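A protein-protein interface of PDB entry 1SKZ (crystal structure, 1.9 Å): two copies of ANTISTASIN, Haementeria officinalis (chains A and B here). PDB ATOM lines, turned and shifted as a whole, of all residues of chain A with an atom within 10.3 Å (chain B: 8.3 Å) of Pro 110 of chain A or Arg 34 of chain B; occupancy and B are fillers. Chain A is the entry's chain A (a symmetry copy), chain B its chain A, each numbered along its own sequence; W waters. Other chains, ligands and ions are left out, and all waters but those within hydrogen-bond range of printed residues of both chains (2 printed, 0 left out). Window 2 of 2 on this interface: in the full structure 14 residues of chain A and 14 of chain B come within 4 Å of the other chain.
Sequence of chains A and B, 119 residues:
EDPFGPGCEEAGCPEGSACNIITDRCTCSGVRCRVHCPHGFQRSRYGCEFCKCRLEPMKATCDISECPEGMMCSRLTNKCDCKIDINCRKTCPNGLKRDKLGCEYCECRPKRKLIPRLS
Hydrophobic or aromatic side chains of chain B that line the printed part of chain A: Val 35. Along chain A the printed residues that touch a printed residue of chain B span positions 44 to 110. Among the printed residues, 5 pairs touch across the chains.
O of Cys 51 of chain B touches CB of Ser 44 of chain A (3.2 Å). Val 35 of chain B touches Arg 45 of chain A (CG1 to NH2, 3.6 Å).
Water W1 bridges the backbone carbonyl oxygen (O) of His 36 of chain B (2.6 Å) and the guanidinium group (NH2) of Arg 45 of chain A (3.4 Å). Water W2 bridges N of Arg 34 of chain B (3.1 Å) and NE of Arg 109 of chain A (3.5 Å).
Of chain B, only Arg 34 comes within 4 Å of Pro 110 of chain A. Arg 34 of chain B touches one residue of chain A. No residue of chain A comes within 4 Å of Cys 33 of chain B. Of the printed residues of chain B, Ser 44 of chain A touches Cys 51 (3.2 Å). Of the printed residues of chain B, Arg 109 of chain A touches Arg 32 (3.4 Å). Of the printed residues of chain A, Arg 32 of chain B touches Arg 109. Of the printed residues of chain B, Arg 45 of chain A touches Val 35 and Cys 51. Val 31 of chain B touches none of the printed residues of chain A. Glu 107 of chain A touches none of the printed residues of chain B. The nearest residue of chain B that does not touch Pro 110 of chain A is Val 35 of chain B (6.2 Å). The nearest residue of chain A that does not touch Arg 34 of chain B is Asn 94 of chain A (5.0 Å).
The guanidinium group (NH2) of Arg 109 of chain A lies within hydrogen-bond range of the backbone carbonyl oxygen (O) of Arg 32 of chain B, at 3.4 Å. NH1 of Arg 34 of chain B is in hydrogen-bond range of O of Pro 110 of chain A (3.1 Å). O of Cys 51 of chain B sits at hydrogen-bond distance from N of Arg 45 of chain A.
No position is printed for both chains.
SG of Cys 33 of chain B sits at hydrogen-bond distance from N of Val 35 of chain B, at 3.5 Å. The side-chain sulfur (SG) of Cys 33 of chain B forms a disulfide with the side-chain sulfur (SG) of Cys 51 of chain B, at 2.0 Å. The backbone carbonyl oxygen (O) of Arg 109 of chain A is in hydrogen-bond range of the side-chain amide nitrogen (ND2) of Asn 94 of chain A (3.2 Å). The side-chain amide nitrogen (ND2) of Asn 94 of chain A sits at hydrogen-bond distance from the backbone carbonyl oxygen (O) of Pro 110 of chain A (3.1 Å). The backbone carbonyl oxygen (O) of Gly 95 of chain A lies within hydrogen-bond range of the backbone NH (N) of Arg 109 of chain A (2.8 Å). The side-chain sulfur (SG) of Cys 108 of chain A forms a disulfide with the side-chain sulfur (SG) of Cys 92 of chain A (2.0 Å).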
ATOM      1  N   SER A  44      -0.249  18.123   2.620  1.00  0.00           N
ATOM      2  CA  SER A  44      -1.251  17.399   3.396  1.00  0.00           C
ATOM      3  C   SER A  44      -2.308  16.793   2.471  1.00  0.00           C
ATOM      4  O   SER A  44      -2.461  17.196   1.303  1.00  0.00           O
ATOM      5  CB  SER A  44      -1.921  18.332   4.416  1.00  0.00           C
ATOM      6  OG  SER A  44      -2.596  19.381   3.756  1.00  0.00           O
ATOM      7  N   ARG A  45      -2.979  15.760   2.967  1.00  0.00           N
ATOM      8  CA  ARG A  45      -4.003  15.072   2.168  1.00  0.00           C
ATOM      9  C   ARG A  45      -5.188  16.012   1.874  1.00  0.00           C
ATOM     10  O   ARG A  45      -6.024  15.695   1.015  1.00  0.00           O
ATOM     11  CB  ARG A  45      -4.518  13.829   2.884  1.00  0.00           C
ATOM     12  CG  ARG A  45      -5.148  14.090   4.250  1.00  0.00           C
ATOM     13  CD  ARG A  45      -6.009  12.919   4.613  1.00  0.00           C
ATOM     14  NE  ARG A  45      -5.242  11.791   5.141  1.00  0.00           N
ATOM     15  CZ  ARG A  45      -5.688  10.543   5.197  1.00  0.00           C
ATOM     16  NH1 ARG A  45      -6.973  10.353   5.456  1.00  0.00           N
ATOM     17  NH2 ARG A  45      -4.853   9.566   5.561  1.00  0.00           N
ATOM     18  N   TYR A  46      -5.299  17.112   2.638  1.00  0.00           N
ATOM     19  CA  TYR A  46      -6.326  18.119   2.346  1.00  0.00           C
ATOM     20  C   TYR A  46      -5.856  19.226   1.424  1.00  0.00           C
ATOM     21  O   TYR A  46      -6.608  20.144   1.172  1.00  0.00           O
ATOM     22  CB  TYR A  46      -6.905  18.704   3.635  1.00  0.00           C
ATOM     23  CG  TYR A  46      -7.866  17.726   4.333  1.00  0.00           C
ATOM     24  CD1 TYR A  46      -9.144  17.474   3.800  1.00  0.00           C
ATOM     25  CD2 TYR A  46      -7.456  16.984   5.459  1.00  0.00           C
ATOM     26  CE1 TYR A  46      -9.977  16.509   4.346  1.00  0.00           C
ATOM     27  CE2 TYR A  46      -8.297  16.008   6.021  1.00  0.00           C
ATOM     28  CZ  TYR A  46      -9.560  15.773   5.447  1.00  0.00           C
ATOM     29  OH  TYR A  46     -10.391  14.786   5.954  1.00  0.00           O
ATOM     30  N   THR A  91     -25.024  14.610   5.646  1.00  0.00           N
ATOM     31  CA  THR A  91     -24.842  16.021   5.888  1.00  0.00           C
ATOM     32  C   THR A  91     -23.811  16.153   7.018  1.00  0.00           C
ATOM     33  O   THR A  91     -23.829  15.422   8.022  1.00  0.00           O
ATOM     34  CB  THR A  91     -26.211  16.679   6.275  1.00  0.00           C
ATOM     35  OG1 THR A  91     -27.156  16.460   5.206  1.00  0.00           O
ATOM     36  CG2 THR A  91     -26.052  18.192   6.531  1.00  0.00           C
ATOM     37  N   CYS A  92     -22.832  17.000   6.773  1.00  0.00           N
ATOM     38  CA  CYS A  92     -21.720  17.176   7.682  1.00  0.00           C
ATOM     39  C   CYS A  92     -21.533  18.696   7.748  1.00  0.00           C
ATOM     40  O   CYS A  92     -21.719  19.371   6.740  1.00  0.00           O
ATOM     41  CB  CYS A  92     -20.472  16.488   7.095  1.00  0.00           C
ATOM     42  SG  CYS A  92     -20.666  14.731   6.584  1.00  0.00           S
ATOM     43  N   PRO A  93     -21.283  19.261   8.958  1.00  0.00           N
ATOM     44  CA  PRO A  93     -20.764  20.634   9.120  1.00  0.00           C
ATOM     45  C   PRO A  93     -19.345  20.826   8.577  1.00  0.00           C
ATOM     46  O   PRO A  93     -19.069  21.794   7.858  1.00  0.00           O
ATOM     47  CB  PRO A  93     -20.793  20.835  10.625  1.00  0.00           C
ATOM     48  CG  PRO A  93     -20.541  19.438  11.180  1.00  0.00           C
ATOM     49  CD  PRO A  93     -21.388  18.573  10.261  1.00  0.00           C
ATOM     50  N   ASN A  94     -18.437  19.932   8.972  1.00  0.00           N
ATOM     51  CA  ASN A  94     -17.043  20.015   8.532  1.00  0.00           C
ATOM     52  C   ASN A  94     -16.868  19.540   7.096  1.00  0.00           C
ATOM     53  O   ASN A  94     -15.751  19.542   6.584  1.00  0.00           O
ATOM     54  CB  ASN A  94     -16.136  19.152   9.412  1.00  0.00           C
ATOM     55  CG  ASN A  94     -15.805  19.796  10.740  1.00  0.00           C
ATOM     56  OD1 ASN A  94     -16.240  20.917  11.036  1.00  0.00           O
ATOM     57  ND2 ASN A  94     -15.022  19.084  11.555  1.00  0.00           N
ATOM     58  N   GLY A  95     -17.917  18.962   6.525  1.00  0.00           N
ATOM     59  CA  GLY A  95     -17.763  18.314   5.232  1.00  0.00           C
ATOM     60  C   GLY A  95     -17.122  16.941   5.349  1.00  0.00           C
ATOM     61  O   GLY A  95     -16.714  16.509   6.451  1.00  0.00           O
ATOM     62  N   LEU A  96     -16.972  16.280   4.208  1.00  0.00           N
ATOM     63  CA  LEU A  96     -16.564  14.880   4.175  1.00  0.00           C
ATOM     64  C   LEU A  96     -15.033  14.679   4.362  1.00  0.00           C
ATOM     65  O   LEU A  96     -14.197  15.482   3.901  1.00  0.00           O
ATOM     66  CB  LEU A  96     -17.008  14.234   2.841  1.00  0.00           C
ATOM     67  CG  LEU A  96     -18.499  13.988   2.493  1.00  0.00           C
ATOM     68  CD1 LEU A  96     -18.606  13.524   1.062  1.00  0.00           C
ATOM     69  CD2 LEU A  96     -19.147  12.974   3.441  1.00  0.00           C
ATOM     70  N   LYS A  97     -14.671  13.532   4.915  1.00  0.00           N
ATOM     71  CA  LYS A  97     -13.257  13.187   5.054  1.00  0.00           C
ATOM     72  C   LYS A  97     -12.653  12.975   3.669  1.00  0.00           C
ATOM     73  O   LYS A  97     -13.315  12.451   2.774  1.00  0.00           O
ATOM     74  CB  LYS A  97     -13.087  11.894   5.880  1.00  0.00           C
ATOM     75  CG  LYS A  97     -13.444  12.019   7.360  1.00  0.00           C
ATOM     76  CD  LYS A  97     -13.177  10.679   8.089  1.00  0.00           C
ATOM     77  CE  LYS A  97     -13.545  10.734   9.589  1.00  0.00           C
ATOM     78  NZ  LYS A  97     -13.535   9.344  10.191  1.00  0.00           N
ATOM     79  N   ARG A  98     -11.361  13.271   3.540  1.00  0.00           N
ATOM     80  CA  ARG A  98     -10.560  12.795   2.418  1.00  0.00           C
ATOM     81  C   ARG A  98      -9.567  11.736   2.894  1.00  0.00           C
ATOM     82  O   ARG A  98      -9.122  11.745   4.052  1.00  0.00           O
ATOM     83  CB  ARG A  98      -9.794  13.955   1.759  1.00  0.00           C
ATOM     84  CG  ARG A  98     -10.732  14.947   1.152  1.00  0.00           C
ATOM     85  CD  ARG A  98     -10.002  15.942   0.344  1.00  0.00           C
ATOM     86  NE  ARG A  98     -10.902  16.946  -0.227  1.00  0.00           N
ATOM     87  CZ  ARG A  98     -11.567  16.802  -1.369  1.00  0.00           C
ATOM     88  NH1 ARG A  98     -11.321  15.793  -2.195  1.00  0.00           N
ATOM     89  NH2 ARG A  98     -12.435  17.739  -1.710  1.00  0.00           N
ATOM     90  N   TYR A 105     -14.608  10.546   0.854  1.00  0.00           N
ATOM     91  CA  TYR A 105     -15.416   9.358   1.048  1.00  0.00           C
ATOM     92  C   TYR A 105     -16.442   9.622   2.123  1.00  0.00           C
ATOM     93  O   TYR A 105     -16.510  10.723   2.659  1.00  0.00           O
ATOM     94  CB  TYR A 105     -14.540   8.131   1.374  1.00  0.00           C
ATOM     95  CG  TYR A 105     -13.711   8.230   2.664  1.00  0.00           C
ATOM     96  CD1 TYR A 105     -12.517   8.946   2.689  1.00  0.00           C
ATOM     97  CD2 TYR A 105     -14.108   7.557   3.829  1.00  0.00           C
ATOM     98  CE1 TYR A 105     -11.734   8.996   3.840  1.00  0.00           C
ATOM     99  CE2 TYR A 105     -13.341   7.607   4.961  1.00  0.00           C
ATOM    100  CZ  TYR A 105     -12.157   8.322   4.961  1.00  0.00           C
ATOM    101  OH  TYR A 105     -11.384   8.339   6.097  1.00  0.00           O
ATOM    102  N   CYS A 106     -17.379   8.688   2.245  1.00  0.00           N
ATOM    103  CA  CYS A 106     -18.618   8.934   2.975  1.00  0.00           C
ATOM    104  C   CYS A 106     -18.504   8.807   4.497  1.00  0.00           C
ATOM    105  O   CYS A 106     -19.111   7.918   5.114  1.00  0.00           O
ATOM    106  CB  CYS A 106     -19.698   8.012   2.429  1.00  0.00           C
ATOM    107  SG  CYS A 106     -21.361   8.586   2.805  1.00  0.00           S
ATOM    108  N   GLU A 107     -17.759   9.747   5.081  1.00  0.00           N
ATOM    109  CA  GLU A 107     -17.612   9.924   6.529  1.00  0.00           C
ATOM    110  C   GLU A 107     -17.394  11.411   6.813  1.00  0.00           C
ATOM    111  O   GLU A 107     -16.753  12.118   6.037  1.00  0.00           O
ATOM    112  CB  GLU A 107     -16.435   9.115   7.093  1.00  0.00           C
ATOM    113  CG  GLU A 107     -16.763   7.663   7.310  1.00  0.00           C
ATOM    114  CD  GLU A 107     -15.549   6.834   7.714  1.00  0.00           C
ATOM    115  OE1 GLU A 107     -14.789   7.312   8.594  1.00  0.00           O
ATOM    116  OE2 GLU A 107     -15.369   5.684   7.203  1.00  0.00           O
ATOM    117  N   CYS A 108     -18.101  11.923   7.817  1.00  0.00           N
ATOM    118  CA  CYS A 108     -17.991  13.333   8.154  1.00  0.00           C
ATOM    119  C   CYS A 108     -16.667  13.578   8.830  1.00  0.00           C
ATOM    120  O   CYS A 108     -16.236  12.772   9.673  1.00  0.00           O
ATOM    121  CB  CYS A 108     -19.122  13.766   9.085  1.00  0.00           C
ATOM    122  SG  CYS A 108     -20.765  13.670   8.316  1.00  0.00           S
ATOM    123  N   ARG A 109     -16.060  14.714   8.498  1.00  0.00           N
ATOM    124  CA  ARG A 109     -14.852  15.150   9.178  1.00  0.00           C
ATOM    125  C   ARG A 109     -15.207  15.392  10.620  1.00  0.00           C
ATOM    126  O   ARG A 109     -16.159  16.128  10.917  1.00  0.00           O
ATOM    127  CB  ARG A 109     -14.316  16.455   8.573  1.00  0.00           C
ATOM    128  CG  ARG A 109     -13.484  16.280   7.332  1.00  0.00           C
ATOM    129  CD  ARG A 109     -12.950  17.595   6.845  1.00  0.00           C
ATOM    130  NE  ARG A 109     -11.658  17.926   7.432  1.00  0.00           N
ATOM    131  CZ  ARG A 109     -10.871  18.908   6.990  1.00  0.00           C
ATOM    132  NH1 ARG A 109     -11.238  19.626   5.927  1.00  0.00           N
ATOM    133  NH2 ARG A 109      -9.690  19.140   7.570  1.00  0.00           N
ATOM    134  N   PRO A 110     -14.422  14.815  11.540  1.00  0.00           N
ATOM    135  CA  PRO A 110     -14.575  15.071  12.981  1.00  0.00           C
ATOM    136  C   PRO A 110     -14.272  16.534  13.301  1.00  0.00           C
ATOM    137  O   PRO A 110     -15.095  17.194  13.963  1.00  0.00           O
ATOM    138  CB  PRO A 110     -13.551  14.123  13.625  1.00  0.00           C
ATOM    139  CG  PRO A 110     -13.248  13.089  12.535  1.00  0.00           C
ATOM    140  CD  PRO A 110     -13.316  13.887  11.269  1.00  0.00           C
ATOM    141  N   VAL B  31      -1.575  20.504  13.434  1.00  0.00           N
ATOM    142  CA  VAL B  31      -2.189  19.757  12.346  1.00  0.00           C
ATOM    143  C   VAL B  31      -3.640  20.254  12.177  1.00  0.00           C
ATOM    144  O   VAL B  31      -4.364  20.411  13.156  1.00  0.00           O
ATOM    145  CB  VAL B  31      -2.150  18.241  12.690  1.00  0.00           C
ATOM    146  CG1 VAL B  31      -2.864  17.415  11.635  1.00  0.00           C
ATOM    147  CG2 VAL B  31      -0.705  17.800  12.854  1.00  0.00           C
ATOM    148  N   ARG B  32      -4.036  20.597  10.955  1.00  0.00           N
ATOM    149  CA  ARG B  32      -5.363  21.192  10.789  1.00  0.00           C
ATOM    150  C   ARG B  32      -6.340  20.082  10.468  1.00  0.00           C
ATOM    151  O   ARG B  32      -7.165  20.234   9.589  1.00  0.00           O
ATOM    152  CB  ARG B  32      -5.411  22.236   9.652  1.00  0.00           C
ATOM    153  CG  ARG B  32      -4.557  23.478   9.820  1.00  0.00           C
ATOM    154  CD  ARG B  32      -3.123  23.098   9.524  1.00  0.00           C
ATOM    155  NE  ARG B  32      -2.254  24.158   9.000  1.00  0.00           N
ATOM    156  CZ  ARG B  32      -1.832  25.220   9.689  1.00  0.00           C
ATOM    157  NH1 ARG B  32      -2.549  25.694  10.721  1.00  0.00           N
ATOM    158  NH2 ARG B  32      -0.818  25.932   9.213  1.00  0.00           N
ATOM    159  N   CYS B  33      -6.185  18.927  11.108  1.00  0.00           N
ATOM    160  CA  CYS B  33      -7.078  17.805  10.882  1.00  0.00           C
ATOM    161  C   CYS B  33      -7.067  16.879  12.090  1.00  0.00           C
ATOM    162  O   CYS B  33      -6.217  17.007  13.000  1.00  0.00           O
ATOM    163  CB  CYS B  33      -6.636  17.022   9.656  1.00  0.00           C
ATOM    164  SG  CYS B  33      -5.173  15.963   9.960  1.00  0.00           S
ATOM    165  N   ARG B  34      -7.895  15.843  11.980  1.00  0.00           N
ATOM    166  CA  ARG B  34      -8.048  14.806  12.989  1.00  0.00           C
ATOM    167  C   ARG B  34      -7.923  13.421  12.352  1.00  0.00           C
ATOM    168  O   ARG B  34      -8.486  12.449  12.857  1.00  0.00           O
ATOM    169  CB  ARG B  34      -9.429  14.921  13.662  1.00  0.00           C
ATOM    170  CG  ARG B  34      -9.640  16.195  14.472  1.00  0.00           C
ATOM    171  CD  ARG B  34     -11.029  16.187  15.075  1.00  0.00           C
ATOM    172  NE  ARG B  34     -11.538  17.532  15.358  1.00  0.00           N
ATOM    173  CZ  ARG B  34     -12.674  17.782  16.011  1.00  0.00           C
ATOM    174  NH1 ARG B  34     -13.380  16.783  16.540  1.00  0.00           N
ATOM    175  NH2 ARG B  34     -13.071  19.035  16.186  1.00  0.00           N
ATOM    176  N   VAL B  35      -7.160  13.332  11.273  1.00  0.00           N
ATOM    177  CA  VAL B  35      -6.819  12.048  10.671  1.00  0.00           C
ATOM    178  C   VAL B  35      -6.085  11.139  11.683  1.00  0.00           C
ATOM    179  O   VAL B  35      -5.206  11.610  12.421  1.00  0.00           O
ATOM    180  CB  VAL B  35      -5.933  12.274   9.397  1.00  0.00           C
ATOM    181  CG1 VAL B  35      -5.372  10.963   8.853  1.00  0.00           C
ATOM    182  CG2 VAL B  35      -6.777  12.960   8.322  1.00  0.00           C
ATOM    183  N   HIS B  36      -6.535   9.880  11.775  1.00  0.00           N
ATOM    184  CA  HIS B  36      -5.713   8.774  12.302  1.00  0.00           C
ATOM    185  C   HIS B  36      -4.544   8.308  11.404  1.00  0.00           C
ATOM    186  O   HIS B  36      -4.729   7.709  10.346  1.00  0.00           O
ATOM    187  CB  HIS B  36      -6.598   7.559  12.618  1.00  0.00           C
ATOM    188  CG  HIS B  36      -5.871   6.466  13.343  1.00  0.00           C
ATOM    189  ND1 HIS B  36      -5.402   6.619  14.634  1.00  0.00           N
ATOM    190  CD2 HIS B  36      -5.369   5.286  12.905  1.00  0.00           C
ATOM    191  CE1 HIS B  36      -4.642   5.586  14.953  1.00  0.00           C
ATOM    192  NE2 HIS B  36      -4.598   4.769  13.923  1.00  0.00           N
ATOM    193  N   CYS B  37      -3.326   8.552  11.856  1.00  0.00           N
ATOM    194  CA  CYS B  37      -2.131   8.075  11.173  1.00  0.00           C
ATOM    195  C   CYS B  37      -1.426   7.020  12.036  1.00  0.00           C
ATOM    196  O   CYS B  37      -0.897   7.335  13.113  1.00  0.00           O
ATOM    197  CB  CYS B  37      -1.188   9.227  10.931  1.00  0.00           C
ATOM    198  SG  CYS B  37      -1.813  10.472   9.746  1.00  0.00           S
ATOM    199  N   PHE B  41       2.094  11.689  12.156  1.00  0.00           N
ATOM    200  CA  PHE B  41       2.153  12.721  11.127  1.00  0.00           C
ATOM    201  C   PHE B  41       3.568  12.991  10.681  1.00  0.00           C
ATOM    202  O   PHE B  41       4.498  12.901  11.459  1.00  0.00           O
ATOM    203  CB  PHE B  41       1.562  14.030  11.671  1.00  0.00           C
ATOM    204  CG  PHE B  41       0.080  13.971  11.924  1.00  0.00           C
ATOM    205  CD1 PHE B  41      -0.821  13.752  10.871  1.00  0.00           C
ATOM    206  CD2 PHE B  41      -0.428  14.129  13.215  1.00  0.00           C
ATOM    207  CE1 PHE B  41      -2.181  13.684  11.080  1.00  0.00           C
ATOM    208  CE2 PHE B  41      -1.823  14.059  13.435  1.00  0.00           C
ATOM    209  CZ  PHE B  41      -2.701  13.832  12.334  1.00  0.00           C
ATOM    210  N   CYS B  51      -0.713  17.491   8.278  1.00  0.00           N
ATOM    211  CA  CYS B  51      -1.699  16.419   8.116  1.00  0.00           C
ATOM    212  C   CYS B  51      -1.423  15.523   6.906  1.00  0.00           C
ATOM    213  O   CYS B  51      -2.204  15.480   5.939  1.00  0.00           O
ATOM    214  CB  CYS B  51      -3.123  16.998   8.013  1.00  0.00           C
ATOM    215  SG  CYS B  51      -4.379  15.694   8.101  1.00  0.00           S
HETATM  216  O   HOH W   1      -5.102   7.085   7.872  1.00  0.00           O
HETATM  217  O   HOH W   2     -10.072  15.855   9.704  1.00  0.00           O
